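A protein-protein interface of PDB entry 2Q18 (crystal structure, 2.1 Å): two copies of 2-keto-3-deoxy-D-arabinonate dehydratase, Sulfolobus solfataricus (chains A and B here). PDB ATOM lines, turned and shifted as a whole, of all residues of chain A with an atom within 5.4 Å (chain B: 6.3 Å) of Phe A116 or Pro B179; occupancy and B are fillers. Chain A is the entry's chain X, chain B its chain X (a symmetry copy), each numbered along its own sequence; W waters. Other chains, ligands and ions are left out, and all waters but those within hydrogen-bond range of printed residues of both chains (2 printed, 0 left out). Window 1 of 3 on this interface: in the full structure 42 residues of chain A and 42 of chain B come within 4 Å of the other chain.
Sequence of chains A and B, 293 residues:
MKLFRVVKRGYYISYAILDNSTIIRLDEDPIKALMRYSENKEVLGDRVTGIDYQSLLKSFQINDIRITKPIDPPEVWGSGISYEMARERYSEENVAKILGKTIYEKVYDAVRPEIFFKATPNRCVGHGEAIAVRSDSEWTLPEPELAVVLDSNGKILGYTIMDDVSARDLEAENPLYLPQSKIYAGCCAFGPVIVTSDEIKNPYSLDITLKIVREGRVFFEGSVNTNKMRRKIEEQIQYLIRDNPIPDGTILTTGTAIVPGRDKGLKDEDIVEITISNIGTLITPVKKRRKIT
The backbone NH (N) of Gly A78 lies within hydrogen-bond range of the backbone carbonyl oxygen (O) of Phe A116 (2.8 Å).
The side-chain hydroxyl of Ser A79 lies within hydrogen-bond range of the backbone carbonyl oxygen of Glu A114, at 2.7 Å.
The side-chain carboxylate of Glu A114 lies close to the backbone NH of Gly A80, 3.4 Å away.
The guanidinium group (NH1) of Arg B134 lies within hydrogen-bond range of the backbone carbonyl oxygen (O) of Gln B180 (3.0 Å).
Among the printed residues, merely in contact across the chains: Trp A77 with Ile B183, Glu A114 with Leu B176, Ile A115 with Pro B179, Ile A115 with Gln B180, Phe A116 with Pro B179, Phe A117 with Phe B117 and Phe A117 with Ile B183.
Pro B179 touches two residues of chain A.
Of the printed residues of chain B, Phe A117 touches Phe B117 (3.6 Å) and Ile B183 (3.997 Å).
Printed residues of chain A within 4 Å of Phe B117: Phe A117 (3.6 Å).
Of the printed residues of chain B, Trp A77 touches Ile B183.
Printed residues of chain A within 4 Å of Ile B183: Trp A77 and Phe A117.
Of the printed residues of chain A, Gln B180 touches Ile A115.
Tyr B177 touches none of the printed residues of chain A.
Ser B181 touches none of the printed residues of chain A.
The nearest printed residue of chain B that does not touch Phe A116 is Ile B183 (5.9 Å).
The nearest printed residue of chain A that does not touch Phe B117 is Trp A77 (6.2 Å).
Hydrophobic or aromatic side chains of chain A within 4 Å of the printed part of chain B: Trp A77, Ile A115, Phe A116 and Phe A117.
Of the 12 printed residues of chain B, 5 touch a printed residue of chain A.
Printed residues of chain B that touch a printed residue of chain A: Phe B117, Leu B176, Pro B179, Gln B180 and Ile B183.
Along chain B the printed residues that touch a printed residue of chain A span positions 117 to 183.
Phe A117 touches its own counterpart, Phe B117.
Of the 7 pairs that touch across the chains among the printed residues, 1 has its exchanged pair printed and touching as well.
Water W1 lies within hydrogen-bond range of the backbone carbonyl oxygen of Ile A115 (2.5 Å), the backbone carbonyl oxygen of Leu B176 (2.7 Å) and the side-chain amide nitrogen of Gln B180 (2.9 Å).
Water W2 lies within hydrogen-bond range of O of Leu B176 (2.8 Å) and OE2 of Glu A114 (3.0 Å).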
ATOM      1  N   VAL A  76      -6.176  16.635 -24.206  1.00  0.00           N
ATOM      2  CA  VAL A  76      -6.675  17.898 -24.746  1.00  0.00           C
ATOM      3  C   VAL A  76      -7.212  18.745 -23.602  1.00  0.00           C
ATOM      4  O   VAL A  76      -8.042  18.293 -22.812  1.00  0.00           O
ATOM      5  CB  VAL A  76      -7.773  17.709 -25.830  1.00  0.00           C
ATOM      6  CG1 VAL A  76      -8.188  19.060 -26.402  1.00  0.00           C
ATOM      7  CG2 VAL A  76      -7.284  16.796 -26.950  1.00  0.00           C
ATOM      8  N   TRP A  77      -6.715  19.972 -23.523  1.00  0.00           N
ATOM      9  CA  TRP A  77      -7.131  20.921 -22.506  1.00  0.00           C
ATOM     10  C   TRP A  77      -7.672  22.178 -23.182  1.00  0.00           C
ATOM     11  O   TRP A  77      -7.332  22.481 -24.329  1.00  0.00           O
ATOM     12  CB  TRP A  77      -5.947  21.293 -21.608  1.00  0.00           C
ATOM     13  CG  TRP A  77      -5.456  20.178 -20.718  1.00  0.00           C
ATOM     14  CD1 TRP A  77      -4.688  19.109 -21.085  1.00  0.00           C
ATOM     15  CD2 TRP A  77      -5.686  20.044 -19.310  1.00  0.00           C
ATOM     16  NE1 TRP A  77      -4.425  18.314 -19.990  1.00  0.00           N
ATOM     17  CE2 TRP A  77      -5.026  18.865 -18.888  1.00  0.00           C
ATOM     18  CE3 TRP A  77      -6.376  20.812 -18.359  1.00  0.00           C
ATOM     19  CZ2 TRP A  77      -5.043  18.429 -17.558  1.00  0.00           C
ATOM     20  CZ3 TRP A  77      -6.396  20.378 -17.038  1.00  0.00           C
ATOM     21  CH2 TRP A  77      -5.729  19.197 -16.649  1.00  0.00           C
ATOM     22  N   GLY A  78      -8.505  22.914 -22.458  1.00  0.00           N
ATOM     23  CA  GLY A  78      -9.057  24.145 -22.985  1.00  0.00           C
ATOM     24  C   GLY A  78      -8.910  25.310 -22.036  1.00  0.00           C
ATOM     25  O   GLY A  78      -8.780  25.134 -20.823  1.00  0.00           O
ATOM     26  N   SER A  79      -8.900  26.505 -22.611  1.00  0.00           N
ATOM     27  CA  SER A  79      -9.028  27.731 -21.854  1.00  0.00           C
ATOM     28  C   SER A  79     -10.280  28.442 -22.357  1.00  0.00           C
ATOM     29  O   SER A  79     -10.737  28.206 -23.480  1.00  0.00           O
ATOM     30  CB  SER A  79      -7.790  28.607 -22.031  1.00  0.00           C
ATOM     31  OG  SER A  79      -7.638  29.498 -20.934  1.00  0.00           O
ATOM     32  N   GLY A  80     -10.860  29.279 -21.512  1.00  0.00           N
ATOM     33  CA  GLY A  80     -12.030  30.057 -21.890  1.00  0.00           C
ATOM     34  C   GLY A  80     -11.929  31.457 -21.334  1.00  0.00           C
ATOM     35  O   GLY A  80     -11.044  31.745 -20.516  1.00  0.00           O
ATOM     36  N   GLU A 114      -9.013  30.565 -16.730  1.00  0.00           N
ATOM     37  CA  GLU A 114      -9.722  29.296 -16.681  1.00  0.00           C
ATOM     38  C   GLU A 114      -8.976  28.251 -17.508  1.00  0.00           C
ATOM     39  O   GLU A 114      -8.618  28.502 -18.660  1.00  0.00           O
ATOM     40  CB  GLU A 114     -11.149  29.450 -17.203  1.00  0.00           C
ATOM     41  CG  GLU A 114     -11.973  28.170 -17.115  1.00  0.00           C
ATOM     42  CD  GLU A 114     -13.195  28.191 -18.006  1.00  0.00           C
ATOM     43  OE1 GLU A 114     -13.177  28.901 -19.030  1.00  0.00           O
ATOM     44  OE2 GLU A 114     -14.173  27.492 -17.679  1.00  0.00           O
ATOM     45  N   ILE A 115      -8.733  27.093 -16.900  1.00  0.00           N
ATOM     46  CA  ILE A 115      -8.114  25.945 -17.571  1.00  0.00           C
ATOM     47  C   ILE A 115      -8.948  24.716 -17.226  1.00  0.00           C
ATOM     48  O   ILE A 115      -9.217  24.460 -16.051  1.00  0.00           O
ATOM     49  CB  ILE A 115      -6.646  25.720 -17.088  1.00  0.00           C
ATOM     50  CG1 ILE A 115      -5.725  26.894 -17.469  1.00  0.00           C
ATOM     51  CG2 ILE A 115      -6.080  24.377 -17.583  1.00  0.00           C
ATOM     52  CD1 ILE A 115      -5.463  27.077 -18.965  1.00  0.00           C
ATOM     53  N   PHE A 116      -9.373  23.966 -18.244  1.00  0.00           N
ATOM     54  CA  PHE A 116     -10.150  22.745 -18.014  1.00  0.00           C
ATOM     55  C   PHE A 116      -9.668  21.589 -18.888  1.00  0.00           C
ATOM     56  O   PHE A 116      -9.081  21.809 -19.943  1.00  0.00           O
ATOM     57  CB  PHE A 116     -11.656  22.999 -18.215  1.00  0.00           C
ATOM     58  CG  PHE A 116     -12.015  23.514 -19.590  1.00  0.00           C
ATOM     59  CD1 PHE A 116     -12.337  22.629 -20.619  1.00  0.00           C
ATOM     60  CD2 PHE A 116     -12.044  24.883 -19.850  1.00  0.00           C
ATOM     61  CE1 PHE A 116     -12.668  23.099 -21.893  1.00  0.00           C
ATOM     62  CE2 PHE A 116     -12.374  25.366 -21.123  1.00  0.00           C
ATOM     63  CZ  PHE A 116     -12.686  24.471 -22.144  1.00  0.00           C
ATOM     64  N   PHE A 117      -9.908  20.362 -18.439  1.00  0.00           N
ATOM     65  CA  PHE A 117      -9.626  19.180 -19.249  1.00  0.00           C
ATOM     66  C   PHE A 117     -10.764  19.002 -20.253  1.00  0.00           C
ATOM     67  O   PHE A 117     -11.937  19.002 -19.874  1.00  0.00           O
ATOM     68  CB  PHE A 117      -9.492  17.932 -18.366  1.00  0.00           C
ATOM     69  CG  PHE A 117      -9.072  16.693 -19.121  1.00  0.00           C
ATOM     70  CD1 PHE A 117     -10.021  15.763 -19.546  1.00  0.00           C
ATOM     71  CD2 PHE A 117      -7.729  16.455 -19.406  1.00  0.00           C
ATOM     72  CE1 PHE A 117      -9.638  14.611 -20.246  1.00  0.00           C
ATOM     73  CE2 PHE A 117      -7.335  15.312 -20.105  1.00  0.00           C
ATOM     74  CZ  PHE A 117      -8.292  14.389 -20.527  1.00  0.00           C
ATOM     75  N   LYS A 118     -10.410  18.835 -21.524  1.00  0.00           N
ATOM     76  CA  LYS A 118     -11.401  18.789 -22.600  1.00  0.00           C
ATOM     77  C   LYS A 118     -11.660  17.381 -23.139  1.00  0.00           C
ATOM     78  O   LYS A 118     -12.814  16.954 -23.223  1.00  0.00           O
ATOM     79  CB  LYS A 118     -11.007  19.748 -23.734  1.00  0.00           C
ATOM     80  CG  LYS A 118     -11.874  19.654 -25.004  1.00  0.00           C
ATOM     81  CD  LYS A 118     -13.351  19.950 -24.725  1.00  0.00           C
ATOM     82  CE  LYS A 118     -14.202  19.658 -25.954  1.00  0.00           C
ATOM     83  NZ  LYS A 118     -15.657  19.929 -25.703  1.00  0.00           N
ATOM     84  N   ASP A 164     -14.308  23.238 -29.835  1.00  0.00           N
ATOM     85  CA  ASP A 164     -14.663  22.843 -28.477  1.00  0.00           C
ATOM     86  C   ASP A 164     -16.187  22.751 -28.398  1.00  0.00           C
ATOM     87  O   ASP A 164     -16.860  23.721 -28.046  1.00  0.00           O
ATOM     88  CB  ASP A 164     -14.090  23.853 -27.458  1.00  0.00           C
ATOM     89  CG  ASP A 164     -14.498  23.556 -26.012  1.00  0.00           C
ATOM     90  OD1 ASP A 164     -15.198  22.554 -25.748  1.00  0.00           O
ATOM     91  OD2 ASP A 164     -14.119  24.346 -25.120  1.00  0.00           O
ATOM     92  N   LEU A 178     -19.999  21.782 -15.912  1.00  0.00           N
ATOM     93  CA  LEU A 178     -19.082  22.067 -17.017  1.00  0.00           C
ATOM     94  C   LEU A 178     -18.377  20.829 -17.602  1.00  0.00           C
ATOM     95  O   LEU A 178     -18.343  20.680 -18.823  1.00  0.00           O
ATOM     96  CB  LEU A 178     -18.064  23.158 -16.651  1.00  0.00           C
ATOM     97  CG  LEU A 178     -17.301  23.763 -17.840  1.00  0.00           C
ATOM     98  CD1 LEU A 178     -18.193  24.692 -18.664  1.00  0.00           C
ATOM     99  CD2 LEU A 178     -16.049  24.498 -17.382  1.00  0.00           C
ATOM    100  N   LYS A 182     -18.685  19.367 -21.510  1.00  0.00           N
ATOM    101  CA  LYS A 182     -17.458  19.468 -22.308  1.00  0.00           C
ATOM    102  C   LYS A 182     -16.856  18.134 -22.746  1.00  0.00           C
ATOM    103  O   LYS A 182     -16.214  18.074 -23.791  1.00  0.00           O
ATOM    104  CB  LYS A 182     -16.384  20.247 -21.539  1.00  0.00           C
ATOM    105  CG  LYS A 182     -16.668  21.731 -21.340  1.00  0.00           C
ATOM    106  CD  LYS A 182     -16.327  22.538 -22.569  1.00  0.00           C
ATOM    107  CE  LYS A 182     -16.498  24.023 -22.306  1.00  0.00           C
ATOM    108  NZ  LYS A 182     -16.210  24.810 -23.540  1.00  0.00           N
ATOM    109  N   PHE B 117     -13.885  15.071 -14.336  1.00  0.00           N
ATOM    110  CA  PHE B 117     -12.685  14.290 -14.622  1.00  0.00           C
ATOM    111  C   PHE B 117     -11.644  14.597 -13.546  1.00  0.00           C
ATOM    112  O   PHE B 117     -11.351  15.763 -13.274  1.00  0.00           O
ATOM    113  CB  PHE B 117     -12.132  14.627 -16.013  1.00  0.00           C
ATOM    114  CG  PHE B 117     -10.964  13.763 -16.431  1.00  0.00           C
ATOM    115  CD1 PHE B 117      -9.654  14.214 -16.273  1.00  0.00           C
ATOM    116  CD2 PHE B 117     -11.175  12.502 -16.983  1.00  0.00           C
ATOM    117  CE1 PHE B 117      -8.567  13.418 -16.659  1.00  0.00           C
ATOM    118  CE2 PHE B 117     -10.100  11.698 -17.369  1.00  0.00           C
ATOM    119  CZ  PHE B 117      -8.793  12.158 -17.206  1.00  0.00           C
ATOM    120  N   ARG B 134      -0.431  21.600  -4.461  1.00  0.00           N
ATOM    121  CA  ARG B 134       0.008  22.538  -5.491  1.00  0.00           C
ATOM    122  C   ARG B 134       0.842  23.662  -4.870  1.00  0.00           C
ATOM    123  O   ARG B 134       0.567  24.099  -3.750  1.00  0.00           O
ATOM    124  CB  ARG B 134      -1.203  23.141  -6.218  1.00  0.00           C
ATOM    125  CG  ARG B 134      -1.990  22.172  -7.118  1.00  0.00           C
ATOM    126  CD  ARG B 134      -3.181  22.883  -7.788  1.00  0.00           C
ATOM    127  NE  ARG B 134      -2.719  24.058  -8.522  1.00  0.00           N
ATOM    128  CZ  ARG B 134      -2.625  24.148  -9.843  1.00  0.00           C
ATOM    129  NH1 ARG B 134      -3.016  23.144 -10.627  1.00  0.00           N
ATOM    130  NH2 ARG B 134      -2.161  25.266 -10.382  1.00  0.00           N
ATOM    131  N   PRO B 175     -15.727  28.585  -9.092  1.00  0.00           N
ATOM    132  CA  PRO B 175     -16.048  27.214  -9.527  1.00  0.00           C
ATOM    133  C   PRO B 175     -15.418  26.840 -10.871  1.00  0.00           C
ATOM    134  O   PRO B 175     -15.267  25.653 -11.171  1.00  0.00           O
ATOM    135  CB  PRO B 175     -17.576  27.224  -9.643  1.00  0.00           C
ATOM    136  CG  PRO B 175     -17.963  28.672  -9.712  1.00  0.00           C
ATOM    137  CD  PRO B 175     -16.944  29.393  -8.892  1.00  0.00           C
ATOM    138  N   LEU B 176     -15.045  27.847 -11.659  1.00  0.00           N
ATOM    139  CA  LEU B 176     -14.377  27.636 -12.939  1.00  0.00           C
ATOM    140  C   LEU B 176     -12.913  27.217 -12.778  1.00  0.00           C
ATOM    141  O   LEU B 176     -12.263  26.833 -13.757  1.00  0.00           O
ATOM    142  CB  LEU B 176     -14.487  28.888 -13.821  1.00  0.00           C
ATOM    143  CG  LEU B 176     -15.900  29.319 -14.253  1.00  0.00           C
ATOM    144  CD1 LEU B 176     -15.835  30.584 -15.091  1.00  0.00           C
ATOM    145  CD2 LEU B 176     -16.631  28.207 -15.013  1.00  0.00           C
ATOM    146  N   TYR B 177     -12.399  27.301 -11.550  1.00  0.00           N
ATOM    147  CA  TYR B 177     -11.041  26.843 -11.239  1.00  0.00           C
ATOM    148  C   TYR B 177     -11.012  25.397 -10.734  1.00  0.00           C
ATOM    149  O   TYR B 177      -9.944  24.872 -10.404  1.00  0.00           O
ATOM    150  CB  TYR B 177     -10.372  27.754 -10.201  1.00  0.00           C
ATOM    151  CG  TYR B 177     -10.133  29.188 -10.634  1.00  0.00           C
ATOM    152  CD1 TYR B 177      -9.839  29.507 -11.959  1.00  0.00           C
ATOM    153  CD2 TYR B 177     -10.164  30.224  -9.698  1.00  0.00           C
ATOM    154  CE1 TYR B 177      -9.612  30.825 -12.351  1.00  0.00           C
ATOM    155  CE2 TYR B 177      -9.937  31.548 -10.077  1.00  0.00           C
ATOM    156  CZ  TYR B 177      -9.661  31.841 -11.402  1.00  0.00           C
ATOM    157  OH  TYR B 177      -9.433  33.146 -11.778  1.00  0.00           O
ATOM    158  N   LEU B 178     -12.178  24.758 -10.666  1.00  0.00           N
ATOM    159  CA  LEU B 178     -12.274  23.385 -10.168  1.00  0.00           C
ATOM    160  C   LEU B 178     -11.296  22.394 -10.827  1.00  0.00           C
ATOM    161  O   LEU B 178     -10.643  21.633 -10.114  1.00  0.00           O
ATOM    162  CB  LEU B 178     -13.714  22.855 -10.222  1.00  0.00           C
ATOM    163  CG  LEU B 178     -13.968  21.575  -9.410  1.00  0.00           C
ATOM    164  CD1 LEU B 178     -13.994  21.860  -7.908  1.00  0.00           C
ATOM    165  CD2 LEU B 178     -15.257  20.889  -9.841  1.00  0.00           C
ATOM    166  N   PRO B 179     -11.190  22.394 -12.179  1.00  0.00           N
ATOM    167  CA  PRO B 179     -10.214  21.484 -12.812  1.00  0.00           C
ATOM    168  C   PRO B 179      -8.778  21.677 -12.302  1.00  0.00           C
ATOM    169  O   PRO B 179      -8.094  20.691 -12.020  1.00  0.00           O
ATOM    170  CB  PRO B 179     -10.311  21.841 -14.301  1.00  0.00           C
ATOM    171  CG  PRO B 179     -11.691  22.395 -14.463  1.00  0.00           C
ATOM    172  CD  PRO B 179     -11.952  23.157 -13.192  1.00  0.00           C
ATOM    173  N   GLN B 180      -8.341  22.930 -12.183  1.00  0.00           N
ATOM    174  CA  GLN B 180      -7.023  23.256 -11.642  1.00  0.00           C
ATOM    175  C   GLN B 180      -6.872  22.795 -10.191  1.00  0.00           C
ATOM    176  O   GLN B 180      -5.789  22.382  -9.776  1.00  0.00           O
ATOM    177  CB  GLN B 180      -6.752  24.760 -11.731  1.00  0.00           C
ATOM    178  CG  GLN B 180      -6.464  25.267 -13.128  1.00  0.00           C
ATOM    179  CD  GLN B 180      -6.204  26.759 -13.156  1.00  0.00           C
ATOM    180  OE1 GLN B 180      -5.112  27.219 -12.810  1.00  0.00           O
ATOM    181  NE2 GLN B 180      -7.205  27.527 -13.579  1.00  0.00           N
ATOM    182  N   SER B 181      -7.967  22.862  -9.438  1.00  0.00           N
ATOM    183  CA  SER B 181      -7.966  22.470  -8.034  1.00  0.00           C
ATOM    184  C   SER B 181      -7.949  20.951  -7.860  1.00  0.00           C
ATOM    185  O   SER B 181      -7.657  20.454  -6.765  1.00  0.00           O
ATOM    186  CB  SER B 181      -9.182  23.059  -7.322  1.00  0.00           C
ATOM    187  OG  SER B 181     -10.332  22.261  -7.534  1.00  0.00           O
ATOM    188  N   LYS B 182      -8.252  20.231  -8.942  1.00  0.00           N
ATOM    189  CA  LYS B 182      -8.459  18.779  -8.897  1.00  0.00           C
ATOM    190  C   LYS B 182      -7.429  17.952  -9.665  1.00  0.00           C
ATOM    191  O   LYS B 182      -7.167  16.813  -9.289  1.00  0.00           O
ATOM    192  CB  LYS B 182      -9.852  18.422  -9.431  1.00  0.00           C
ATOM    193  CG  LYS B 182     -11.020  18.862  -8.556  1.00  0.00           C
ATOM    194  CD  LYS B 182     -11.252  17.911  -7.408  1.00  0.00           C
ATOM    195  CE  LYS B 182     -12.494  18.298  -6.627  1.00  0.00           C
ATOM    196  NZ  LYS B 182     -12.687  17.385  -5.463  1.00  0.00           N
ATOM    197  N   ILE B 183      -6.877  18.512 -10.741  1.00  0.00           N
ATOM    198  CA  ILE B 183      -6.067  17.742 -11.700  1.00  0.00           C
ATOM    199  C   ILE B 183      -4.630  18.252 -11.776  1.00  0.00           C
ATOM    200  O   ILE B 183      -4.372  19.334 -12.306  1.00  0.00           O
ATOM    201  CB  ILE B 183      -6.690  17.739 -13.142  1.00  0.00           C
ATOM    202  CG1 ILE B 183      -8.203  17.476 -13.098  1.00  0.00           C
ATOM    203  CG2 ILE B 183      -5.981  16.707 -14.041  1.00  0.00           C
ATOM    204  CD1 ILE B 183      -8.943  17.804 -14.409  1.00  0.00           C
ATOM    205  N   TYR B 184      -3.703  17.450 -11.255  1.00  0.00           N
ATOM    206  CA  TYR B 184      -2.277  17.790 -11.219  1.00  0.00           C
ATOM    207  C   TYR B 184      -1.477  16.574 -10.734  1.00  0.00           C
ATOM    208  O   TYR B 184      -2.064  15.586 -10.291  1.00  0.00           O
ATOM    209  CB  TYR B 184      -2.030  19.025 -10.329  1.00  0.00           C
ATOM    210  CG  TYR B 184      -2.514  18.872  -8.901  1.00  0.00           C
ATOM    211  CD1 TYR B 184      -1.662  18.388  -7.908  1.00  0.00           C
ATOM    212  CD2 TYR B 184      -3.817  19.215  -8.541  1.00  0.00           C
ATOM    213  CE1 TYR B 184      -2.100  18.234  -6.594  1.00  0.00           C
ATOM    214  CE2 TYR B 184      -4.264  19.068  -7.225  1.00  0.00           C
ATOM    215  CZ  TYR B 184      -3.394  18.580  -6.261  1.00  0.00           C
ATOM    216  OH  TYR B 184      -3.808  18.430  -4.955  1.00  0.00           O
HETATM  217  O   HOH W   1      -9.719  26.197 -14.299  1.00  0.00           O
HETATM  218  O   HOH W   2     -13.274  25.298 -15.842  1.00  0.00           O
